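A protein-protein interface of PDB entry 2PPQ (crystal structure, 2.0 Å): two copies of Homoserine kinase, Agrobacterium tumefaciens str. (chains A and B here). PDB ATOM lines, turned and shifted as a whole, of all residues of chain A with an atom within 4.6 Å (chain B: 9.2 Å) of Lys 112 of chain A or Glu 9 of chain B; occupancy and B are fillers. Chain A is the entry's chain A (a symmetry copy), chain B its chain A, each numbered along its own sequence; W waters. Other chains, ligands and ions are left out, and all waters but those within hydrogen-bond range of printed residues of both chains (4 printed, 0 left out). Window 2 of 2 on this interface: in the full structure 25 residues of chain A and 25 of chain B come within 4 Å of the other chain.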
ATOM      1  N   MET A 108     -10.604   2.611 -10.301  1.00  0.00           N
ATOM      2  CA  MET A 108     -11.046   1.323  -9.825  1.00  0.00           C
ATOM      3  C   MET A 108     -11.716   1.495  -8.475  1.00  0.00           C
ATOM      4  O   MET A 108     -11.390   2.400  -7.722  1.00  0.00           O
ATOM      5  CB  MET A 108      -9.849   0.385  -9.675  1.00  0.00           C
ATOM      6  CG  MET A 108      -8.721   0.947  -8.778  1.00  0.00           C
ATOM      7  SD  MET A 108      -6.900   0.712  -9.613  1.00  0.00           S
ATOM      8  CE  MET A 108      -6.868   2.403 -10.647  1.00  0.00           C
ATOM      9  N   TRP A 109     -12.652   0.614  -8.180  1.00  0.00           N
ATOM     10  CA  TRP A 109     -13.335   0.665  -6.906  1.00  0.00           C
ATOM     11  C   TRP A 109     -12.479  -0.033  -5.860  1.00  0.00           C
ATOM     12  O   TRP A 109     -11.789  -1.017  -6.149  1.00  0.00           O
ATOM     13  CB  TRP A 109     -14.763   0.114  -7.016  1.00  0.00           C
ATOM     14  CG  TRP A 109     -14.925  -1.348  -7.239  1.00  0.00           C
ATOM     15  CD1 TRP A 109     -15.091  -1.984  -8.443  1.00  0.00           C
ATOM     16  CD2 TRP A 109     -15.027  -2.369  -6.229  1.00  0.00           C
ATOM     17  NE1 TRP A 109     -15.268  -3.338  -8.234  1.00  0.00           N
ATOM     18  CE2 TRP A 109     -15.232  -3.590  -6.886  1.00  0.00           C
ATOM     19  CE3 TRP A 109     -14.965  -2.361  -4.834  1.00  0.00           C
ATOM     20  CZ2 TRP A 109     -15.367  -4.789  -6.195  1.00  0.00           C
ATOM     21  CZ3 TRP A 109     -15.093  -3.543  -4.152  1.00  0.00           C
ATOM     22  CH2 TRP A 109     -15.292  -4.743  -4.827  1.00  0.00           C
ATOM     23  N   LEU A 110     -12.523   0.492  -4.647  1.00  0.00           N
ATOM     24  CA  LEU A 110     -11.662   0.048  -3.560  1.00  0.00           C
ATOM     25  C   LEU A 110     -12.210  -1.149  -2.813  1.00  0.00           C
ATOM     26  O   LEU A 110     -13.290  -1.108  -2.211  1.00  0.00           O
ATOM     27  CB  LEU A 110     -11.408   1.217  -2.585  1.00  0.00           C
ATOM     28  CG  LEU A 110     -10.720   2.412  -3.254  1.00  0.00           C
ATOM     29  CD1 LEU A 110     -10.507   3.541  -2.258  1.00  0.00           C
ATOM     30  CD2 LEU A 110      -9.393   1.992  -3.924  1.00  0.00           C
ATOM     31  N   ARG A 111     -11.425  -2.214  -2.829  1.00  0.00           N
ATOM     32  CA  ARG A 111     -11.703  -3.420  -2.035  1.00  0.00           C
ATOM     33  C   ARG A 111     -11.416  -3.214  -0.541  1.00  0.00           C
ATOM     34  O   ARG A 111     -12.124  -3.759   0.301  1.00  0.00           O
ATOM     35  CB  ARG A 111     -10.881  -4.593  -2.561  1.00  0.00           C
ATOM     36  CG  ARG A 111     -11.449  -5.228  -3.825  1.00  0.00           C
ATOM     37  CD  ARG A 111     -11.380  -4.346  -5.062  1.00  0.00           C
ATOM     38  NE  ARG A 111     -11.774  -5.121  -6.233  1.00  0.00           N
ATOM     39  CZ  ARG A 111     -11.976  -4.635  -7.450  1.00  0.00           C
ATOM     40  NH1 ARG A 111     -11.781  -3.359  -7.721  1.00  0.00           N
ATOM     41  NH2 ARG A 111     -12.354  -5.458  -8.423  1.00  0.00           N
ATOM     42  N   LYS A 112     -10.407  -2.405  -0.226  1.00  0.00           N
ATOM     43  CA  LYS A 112     -10.005  -2.151   1.147  1.00  0.00           C
ATOM     44  C   LYS A 112      -9.887  -0.634   1.399  1.00  0.00           C
ATOM     45  O   LYS A 112      -8.775  -0.115   1.590  1.00  0.00           O
ATOM     46  CB  LYS A 112      -8.660  -2.840   1.425  1.00  0.00           C
ATOM     47  CG  LYS A 112      -8.659  -4.372   1.248  1.00  0.00           C
ATOM     48  CD  LYS A 112      -9.607  -5.044   2.251  1.00  0.00           C
ATOM     49  CE  LYS A 112      -9.434  -6.588   2.312  1.00  0.00           C
ATOM     50  NZ  LYS A 112     -10.452  -7.215   3.263  1.00  0.00           N
ATOM     51  N   PRO A 113     -11.028   0.081   1.395  1.00  0.00           N
ATOM     52  CA  PRO A 113     -10.976   1.521   1.611  1.00  0.00           C
ATOM     53  C   PRO A 113     -10.554   1.850   3.035  1.00  0.00           C
ATOM     54  O   PRO A 113     -10.860   1.109   3.987  1.00  0.00           O
ATOM     55  CB  PRO A 113     -12.415   1.978   1.352  1.00  0.00           C
ATOM     56  CG  PRO A 113     -13.252   0.772   1.508  1.00  0.00           C
ATOM     57  CD  PRO A 113     -12.409  -0.396   1.177  1.00  0.00           C
ATOM     58  N   GLU A 114      -9.849   2.955   3.171  1.00  0.00           N
ATOM     59  CA  GLU A 114      -9.319   3.418   4.440  1.00  0.00           C
ATOM     60  C   GLU A 114     -10.076   4.698   4.749  1.00  0.00           C
ATOM     61  O   GLU A 114     -10.787   5.243   3.895  1.00  0.00           O
ATOM     62  CB  GLU A 114      -7.808   3.650   4.346  1.00  0.00           C
ATOM     63  CG  GLU A 114      -7.000   2.397   3.956  1.00  0.00           C
ATOM     64  CD  GLU A 114      -5.615   2.701   3.353  1.00  0.00           C
ATOM     65  OE1 GLU A 114      -5.168   3.869   3.408  1.00  0.00           O
ATOM     66  OE2 GLU A 114      -4.969   1.763   2.814  1.00  0.00           O
ATOM     67  N   LYS A 235     -15.779  -5.488   8.153  1.00  0.00           N
ATOM     68  CA  LYS A 235     -16.290  -6.758   7.630  1.00  0.00           C
ATOM     69  C   LYS A 235     -16.772  -7.678   8.748  1.00  0.00           C
ATOM     70  O   LYS A 235     -17.690  -8.459   8.540  1.00  0.00           O
ATOM     71  CB  LYS A 235     -15.248  -7.438   6.708  1.00  0.00           C
ATOM     72  CG  LYS A 235     -15.262  -6.844   5.295  1.00  0.00           C
ATOM     73  CD  LYS A 235     -14.166  -7.402   4.390  1.00  0.00           C
ATOM     74  CE  LYS A 235     -14.253  -6.822   2.965  1.00  0.00           C
ATOM     75  NZ  LYS A 235     -15.432  -7.356   2.184  1.00  0.00           N
ATOM     76  N   ASP B   6     -11.284 -12.333  -7.148  1.00  0.00           N
ATOM     77  CA  ASP B   6     -11.072 -10.902  -7.253  1.00  0.00           C
ATOM     78  C   ASP B   6      -9.669 -10.554  -6.757  1.00  0.00           C
ATOM     79  O   ASP B   6      -9.022 -11.361  -6.078  1.00  0.00           O
ATOM     80  CB  ASP B   6     -12.136 -10.166  -6.426  1.00  0.00           C
ATOM     81  CG  ASP B   6     -12.222  -8.693  -6.755  1.00  0.00           C
ATOM     82  OD1 ASP B   6     -11.733  -8.300  -7.836  1.00  0.00           O
ATOM     83  OD2 ASP B   6     -12.767  -7.933  -5.927  1.00  0.00           O
ATOM     84  N   ILE B   7      -9.198  -9.359  -7.112  1.00  0.00           N
ATOM     85  CA  ILE B   7      -7.907  -8.845  -6.650  1.00  0.00           C
ATOM     86  C   ILE B   7      -8.095  -7.437  -6.075  1.00  0.00           C
ATOM     87  O   ILE B   7      -8.935  -6.684  -6.562  1.00  0.00           O
ATOM     88  CB  ILE B   7      -6.864  -8.766  -7.800  1.00  0.00           C
ATOM     89  CG1 ILE B   7      -6.825 -10.060  -8.621  1.00  0.00           C
ATOM     90  CG2 ILE B   7      -5.497  -8.510  -7.230  1.00  0.00           C
ATOM     91  CD1 ILE B   7      -6.435 -11.258  -7.811  1.00  0.00           C
ATOM     92  N   THR B   8      -7.297  -7.095  -5.065  1.00  0.00           N
ATOM     93  CA  THR B   8      -7.290  -5.750  -4.478  1.00  0.00           C
ATOM     94  C   THR B   8      -6.338  -4.797  -5.217  1.00  0.00           C
ATOM     95  O   THR B   8      -5.379  -5.225  -5.867  1.00  0.00           O
ATOM     96  CB  THR B   8      -6.916  -5.773  -2.974  1.00  0.00           C
ATOM     97  OG1 THR B   8      -5.495  -5.654  -2.808  1.00  0.00           O
ATOM     98  CG2 THR B   8      -7.408  -7.046  -2.321  1.00  0.00           C
ATOM     99  N   GLU B   9      -6.621  -3.500  -5.107  1.00  0.00           N
ATOM    100  CA  GLU B   9      -5.863  -2.442  -5.793  1.00  0.00           C
ATOM    101  C   GLU B   9      -4.350  -2.433  -5.467  1.00  0.00           C
ATOM    102  O   GLU B   9      -3.488  -2.282  -6.357  1.00  0.00           O
ATOM    103  CB  GLU B   9      -6.488  -1.063  -5.488  1.00  0.00           C
ATOM    104  CG  GLU B   9      -6.761  -0.729  -3.972  1.00  0.00           C
ATOM    105  CD  GLU B   9      -8.046  -1.348  -3.353  1.00  0.00           C
ATOM    106  OE1 GLU B   9      -8.759  -2.114  -4.030  1.00  0.00           O
ATOM    107  OE2 GLU B   9      -8.340  -1.056  -2.164  1.00  0.00           O
ATOM    108  N   ASP B  10      -4.029  -2.627  -4.200  1.00  0.00           N
ATOM    109  CA  ASP B  10      -2.628  -2.590  -3.766  1.00  0.00           C
ATOM    110  C   ASP B  10      -1.860  -3.818  -4.243  1.00  0.00           C
ATOM    111  O   ASP B  10      -0.733  -3.683  -4.699  1.00  0.00           O
ATOM    112  CB  ASP B  10      -2.526  -2.453  -2.249  1.00  0.00           C
ATOM    113  CG  ASP B  10      -2.815  -1.032  -1.765  1.00  0.00           C
ATOM    114  OD1 ASP B  10      -2.627  -0.058  -2.540  1.00  0.00           O
ATOM    115  OD2 ASP B  10      -3.229  -0.894  -0.594  1.00  0.00           O
ATOM    116  N   GLU B  11      -2.485  -4.996  -4.152  1.00  0.00           N
ATOM    117  CA  GLU B  11      -1.893  -6.239  -4.636  1.00  0.00           C
ATOM    118  C   GLU B  11      -1.553  -6.127  -6.122  1.00  0.00           C
ATOM    119  O   GLU B  11      -0.467  -6.506  -6.550  1.00  0.00           O
ATOM    120  CB  GLU B  11      -2.854  -7.428  -4.473  1.00  0.00           C
ATOM    121  CG  GLU B  11      -3.197  -7.870  -3.047  1.00  0.00           C
ATOM    122  CD  GLU B  11      -4.195  -9.060  -3.037  1.00  0.00           C
ATOM    123  OE1 GLU B  11      -5.051  -9.168  -3.968  1.00  0.00           O
ATOM    124  OE2 GLU B  11      -4.115  -9.897  -2.096  1.00  0.00           O
ATOM    125  N   LEU B  12      -2.509  -5.647  -6.912  1.00  0.00           N
ATOM    126  CA  LEU B  12      -2.318  -5.539  -8.360  1.00  0.00           C
ATOM    127  C   LEU B  12      -1.220  -4.504  -8.678  1.00  0.00           C
ATOM    128  O   LEU B  12      -0.355  -4.751  -9.514  1.00  0.00           O
ATOM    129  CB  LEU B  12      -3.647  -5.206  -9.051  1.00  0.00           C
ATOM    130  CG  LEU B  12      -3.677  -5.115 -10.579  1.00  0.00           C
ATOM    131  CD1 LEU B  12      -2.934  -6.246 -11.258  1.00  0.00           C
ATOM    132  CD2 LEU B  12      -5.122  -5.055 -11.094  1.00  0.00           C
ATOM    133  N   ARG B  13      -1.221  -3.365  -7.984  1.00  0.00           N
ATOM    134  CA  ARG B  13      -0.178  -2.367  -8.205  1.00  0.00           C
ATOM    135  C   ARG B  13       1.211  -2.929  -7.883  1.00  0.00           C
ATOM    136  O   ARG B  13       2.146  -2.729  -8.639  1.00  0.00           O
ATOM    137  CB  ARG B  13      -0.445  -1.089  -7.424  1.00  0.00           C
ATOM    138  CG  ARG B  13      -1.481  -0.205  -8.093  1.00  0.00           C
ATOM    139  CD  ARG B  13      -1.559   1.176  -7.441  1.00  0.00           C
ATOM    140  NE  ARG B  13      -2.944   1.623  -7.428  1.00  0.00           N
ATOM    141  CZ  ARG B  13      -3.728   1.701  -6.350  1.00  0.00           C
ATOM    142  NH1 ARG B  13      -4.987   2.105  -6.499  1.00  0.00           N
ATOM    143  NH2 ARG B  13      -3.279   1.404  -5.123  1.00  0.00           N
ATOM    144  N   ASN B  14       1.322  -3.665  -6.788  1.00  0.00           N
ATOM    145  CA  ASN B  14       2.578  -4.332  -6.445  1.00  0.00           C
ATOM    146  C   ASN B  14       2.977  -5.354  -7.504  1.00  0.00           C
ATOM    147  O   ASN B  14       4.134  -5.424  -7.925  1.00  0.00           O
ATOM    148  CB  ASN B  14       2.445  -5.032  -5.103  1.00  0.00           C
ATOM    149  CG  ASN B  14       3.706  -5.757  -4.711  1.00  0.00           C
ATOM    150  OD1 ASN B  14       3.747  -6.995  -4.669  1.00  0.00           O
ATOM    151  ND2 ASN B  14       4.753  -4.998  -4.445  1.00  0.00           N
ATOM    152  N   PHE B  15       2.007  -6.162  -7.922  1.00  0.00           N
ATOM    153  CA  PHE B  15       2.214  -7.120  -9.005  1.00  0.00           C
ATOM    154  C   PHE B  15       2.815  -6.462 -10.270  1.00  0.00           C
ATOM    155  O   PHE B  15       3.733  -7.021 -10.896  1.00  0.00           O
ATOM    156  CB  PHE B  15       0.899  -7.858  -9.316  1.00  0.00           C
ATOM    157  CG  PHE B  15       1.042  -8.949 -10.340  1.00  0.00           C
ATOM    158  CD1 PHE B  15       1.554 -10.189  -9.979  1.00  0.00           C
ATOM    159  CD2 PHE B  15       0.660  -8.741 -11.659  1.00  0.00           C
ATOM    160  CE1 PHE B  15       1.684 -11.186 -10.898  1.00  0.00           C
ATOM    161  CE2 PHE B  15       0.788  -9.757 -12.608  1.00  0.00           C
ATOM    162  CZ  PHE B  15       1.304 -10.980 -12.222  1.00  0.00           C
ATOM    163  N   LEU B  16       2.315  -5.288 -10.638  1.00  0.00           N
ATOM    164  CA  LEU B  16       2.759  -4.631 -11.863  1.00  0.00           C
ATOM    165  C   LEU B  16       4.170  -4.018 -11.777  1.00  0.00           C
ATOM    166  O   LEU B  16       4.761  -3.721 -12.805  1.00  0.00           O
ATOM    167  CB  LEU B  16       1.747  -3.568 -12.323  1.00  0.00           C
ATOM    168  CG  LEU B  16       0.292  -4.001 -12.631  1.00  0.00           C
ATOM    169  CD1 LEU B  16      -0.512  -2.820 -13.177  1.00  0.00           C
ATOM    170  CD2 LEU B  16       0.192  -5.182 -13.572  1.00  0.00           C
ATOM    171  N   LEU B  24      -1.226   1.454 -13.591  1.00  0.00           N
ATOM    172  CA  LEU B  24      -2.623   1.029 -13.621  1.00  0.00           C
ATOM    173  C   LEU B  24      -3.619   2.198 -13.599  1.00  0.00           C
ATOM    174  O   LEU B  24      -3.562   3.055 -12.702  1.00  0.00           O
ATOM    175  CB  LEU B  24      -2.905   0.100 -12.437  1.00  0.00           C
ATOM    176  CG  LEU B  24      -4.236  -0.640 -12.476  1.00  0.00           C
ATOM    177  CD1 LEU B  24      -4.285  -1.524 -13.722  1.00  0.00           C
ATOM    178  CD2 LEU B  24      -4.463  -1.449 -11.195  1.00  0.00           C
ATOM    179  N   TYR B  27      -9.077  -1.619 -13.981  1.00  0.00           N
ATOM    180  CA  TYR B  27      -9.173  -3.056 -14.179  1.00  0.00           C
ATOM    181  C   TYR B  27     -10.577  -3.605 -13.952  1.00  0.00           C
ATOM    182  O   TYR B  27     -11.297  -3.197 -13.034  1.00  0.00           O
ATOM    183  CB  TYR B  27      -8.129  -3.844 -13.382  1.00  0.00           C
ATOM    184  CG  TYR B  27      -8.310  -3.902 -11.893  1.00  0.00           C
ATOM    185  CD1 TYR B  27      -8.858  -5.026 -11.276  1.00  0.00           C
ATOM    186  CD2 TYR B  27      -7.885  -2.853 -11.093  1.00  0.00           C
ATOM    187  CE1 TYR B  27      -9.001  -5.088  -9.890  1.00  0.00           C
ATOM    188  CE2 TYR B  27      -8.019  -2.898  -9.698  1.00  0.00           C
ATOM    189  CZ  TYR B  27      -8.571  -4.014  -9.109  1.00  0.00           C
ATOM    190  OH  TYR B  27      -8.685  -4.029  -7.732  1.00  0.00           O
ATOM    191  N   LEU B  94      -0.742 -14.040  -7.448  1.00  0.00           N
ATOM    192  CA  LEU B  94      -1.718 -13.056  -6.985  1.00  0.00           C
ATOM    193  C   LEU B  94      -2.871 -13.773  -6.316  1.00  0.00           C
ATOM    194  O   LEU B  94      -3.428 -14.721  -6.886  1.00  0.00           O
ATOM    195  CB  LEU B  94      -2.279 -12.234  -8.147  1.00  0.00           C
ATOM    196  CG  LEU B  94      -1.702 -10.863  -8.481  1.00  0.00           C
ATOM    197  CD1 LEU B  94      -2.550 -10.246  -9.605  1.00  0.00           C
ATOM    198  CD2 LEU B  94      -1.647  -9.953  -7.267  1.00  0.00           C
HETATM  199  O   HOH W   1     -12.736  -3.965 -10.889  1.00  0.00           O
HETATM  200  O   HOH W   2      -7.570   0.876  -0.588  1.00  0.00           O
HETATM  201  O   HOH W   3      -9.204  -1.650  -6.804  1.00  0.00           O
HETATM  202  O   HOH W   4     -12.901  -1.355 -10.650  1.00  0.00           O
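OD1 of Asp 6 of chain B is in salt-bridge range of NH2 of Arg 111 of chain A, at 3.0 Å.
NE of Arg 111 of chain A lies within hydrogen-bond range of O of Ile 7 of chain B (3.3 Å).
The side-chain carboxylate (OE1) of Glu 9 of chain B sits at hydrogen-bond distance from the backbone NH (N) of Arg 111 of chain A, at 2.9 Å.
The side-chain carboxylate (OE2) of Glu 9 of chain B is in hydrogen-bond range of the backbone NH (N) of Lys 112 of chain A, 3.1 Å away.
The side-chain hydroxyl of Tyr 27 of chain B sits at hydrogen-bond distance from the guanidinium group of Arg 111 of chain A (3.2 Å).
No position is printed for both chains.
Of the 10 pairs that touch across the chains among the printed residues, none has its exchanged pair printed and touching as well.
Of the printed residues of chain B, Met 108 of chain A touches Arg 13, Leu 24 and Tyr 27.
Of the printed residues of chain B, Trp 109 of chain A touches Glu 9 (3.9 Å).
Of the printed residues of chain B, Arg 111 of chain A touches Asp 6 (3.0 Å), Ile 7 (3.3 Å), Glu 9 (2.9 Å) and Tyr 27 (3.2 Å).
Lys 112 of chain A touches just one residue of chain B: Glu 9.
Thr 8 of chain B touches none of the printed residues of chain A.
Of chain A, only Trp 109 (3.9 Å), Leu 110 (3.6 Å), Arg 111 (2.9 Å) and Lys 112 (3.1 Å) come within 4 Å of Glu 9 of chain B.
Of the printed residues of chain A, Leu 24 of chain B touches Met 108.
The nearest printed residue of chain A that does not touch Tyr 27 of chain B is Trp 109 of chain A (4.6 Å).
Of the 8 printed residues of chain A, 5 touch a printed residue of chain B.
Hydrophobic or aromatic side chains of chain A that line the printed part of chain B: Met 108 and Leu 110.
Along chain A the printed residues that touch a printed residue of chain B span positions 108 to 112.
Of the 14 printed residues of chain B, 6 touch a printed residue of chain A.
Printed residues of chain B that touch a printed residue of chain A: Asp 6, Ile 7, Glu 9, Arg 13, Leu 24 and Tyr 27.
Among the printed residues, 10 pairs touch across the chains.
Among the printed residues, Asp or Glu carboxylates within 4 Å of a Lys or Arg side-chain nitrogen of the other chain: Arg 111 of chain A with Asp 6 of chain B.
Water W3 lies within hydrogen-bond range of the side-chain hydroxyl of Tyr 27 of chain B (2.6 Å), the backbone carbonyl oxygen of Trp 109 of chain A (2.7 Å), the side-chain carboxylate of Glu 9 of chain B (2.8 Å) and the guanidinium group of Arg 111 of chain A (3.2 Å).
Water W2 lies within hydrogen-bond range of OE2 of Glu 9 of chain B (2.6 Å) and O of Lys 112 of chain A (2.7 Å).
Water W1 lies within hydrogen-bond range of O of Tyr 27 of chain B (2.7 Å) and NH2 of Arg 111 of chain A (2.9 Å).
Water W4 bridges the backbone NH (N) of Trp 109 of chain A (3.2 Å) and the backbone carbonyl oxygen (O) of Tyr 27 of chain B (3.4 Å).
O of Ile 7 of chain B lies within hydrogen-bond range of OH of Tyr 27 of chain B (2.9 Å).
The side-chain hydroxyl of Tyr 27 of chain B lies within hydrogen-bond range of the backbone NH of Glu 9 of chain B.
The side-chain carboxylate (OD1) of Asp 10 of chain B is in salt-bridge range of the guanidinium group (NH2) of Arg 13 of chain B, at 3.0 Å.
O of Trp 109 of chain A sits at hydrogen-bond distance from NH1 of Arg 111 of chain A, 2.8 Å away.
Among the printed residues, pairs that only touch across the chains: Met 108 of chain A with Leu 24 of chain B (3.6 Å), Leu 110 of chain A with Glu 9 of chain B (3.6 Å), Met 108 of chain A with Tyr 27 of chain B (3.8 Å), Trp 109 of chain A with Glu 9 of chain B (3.9 Å) and Met 108 of chain A with Arg 13 of chain B (3.9 Å).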
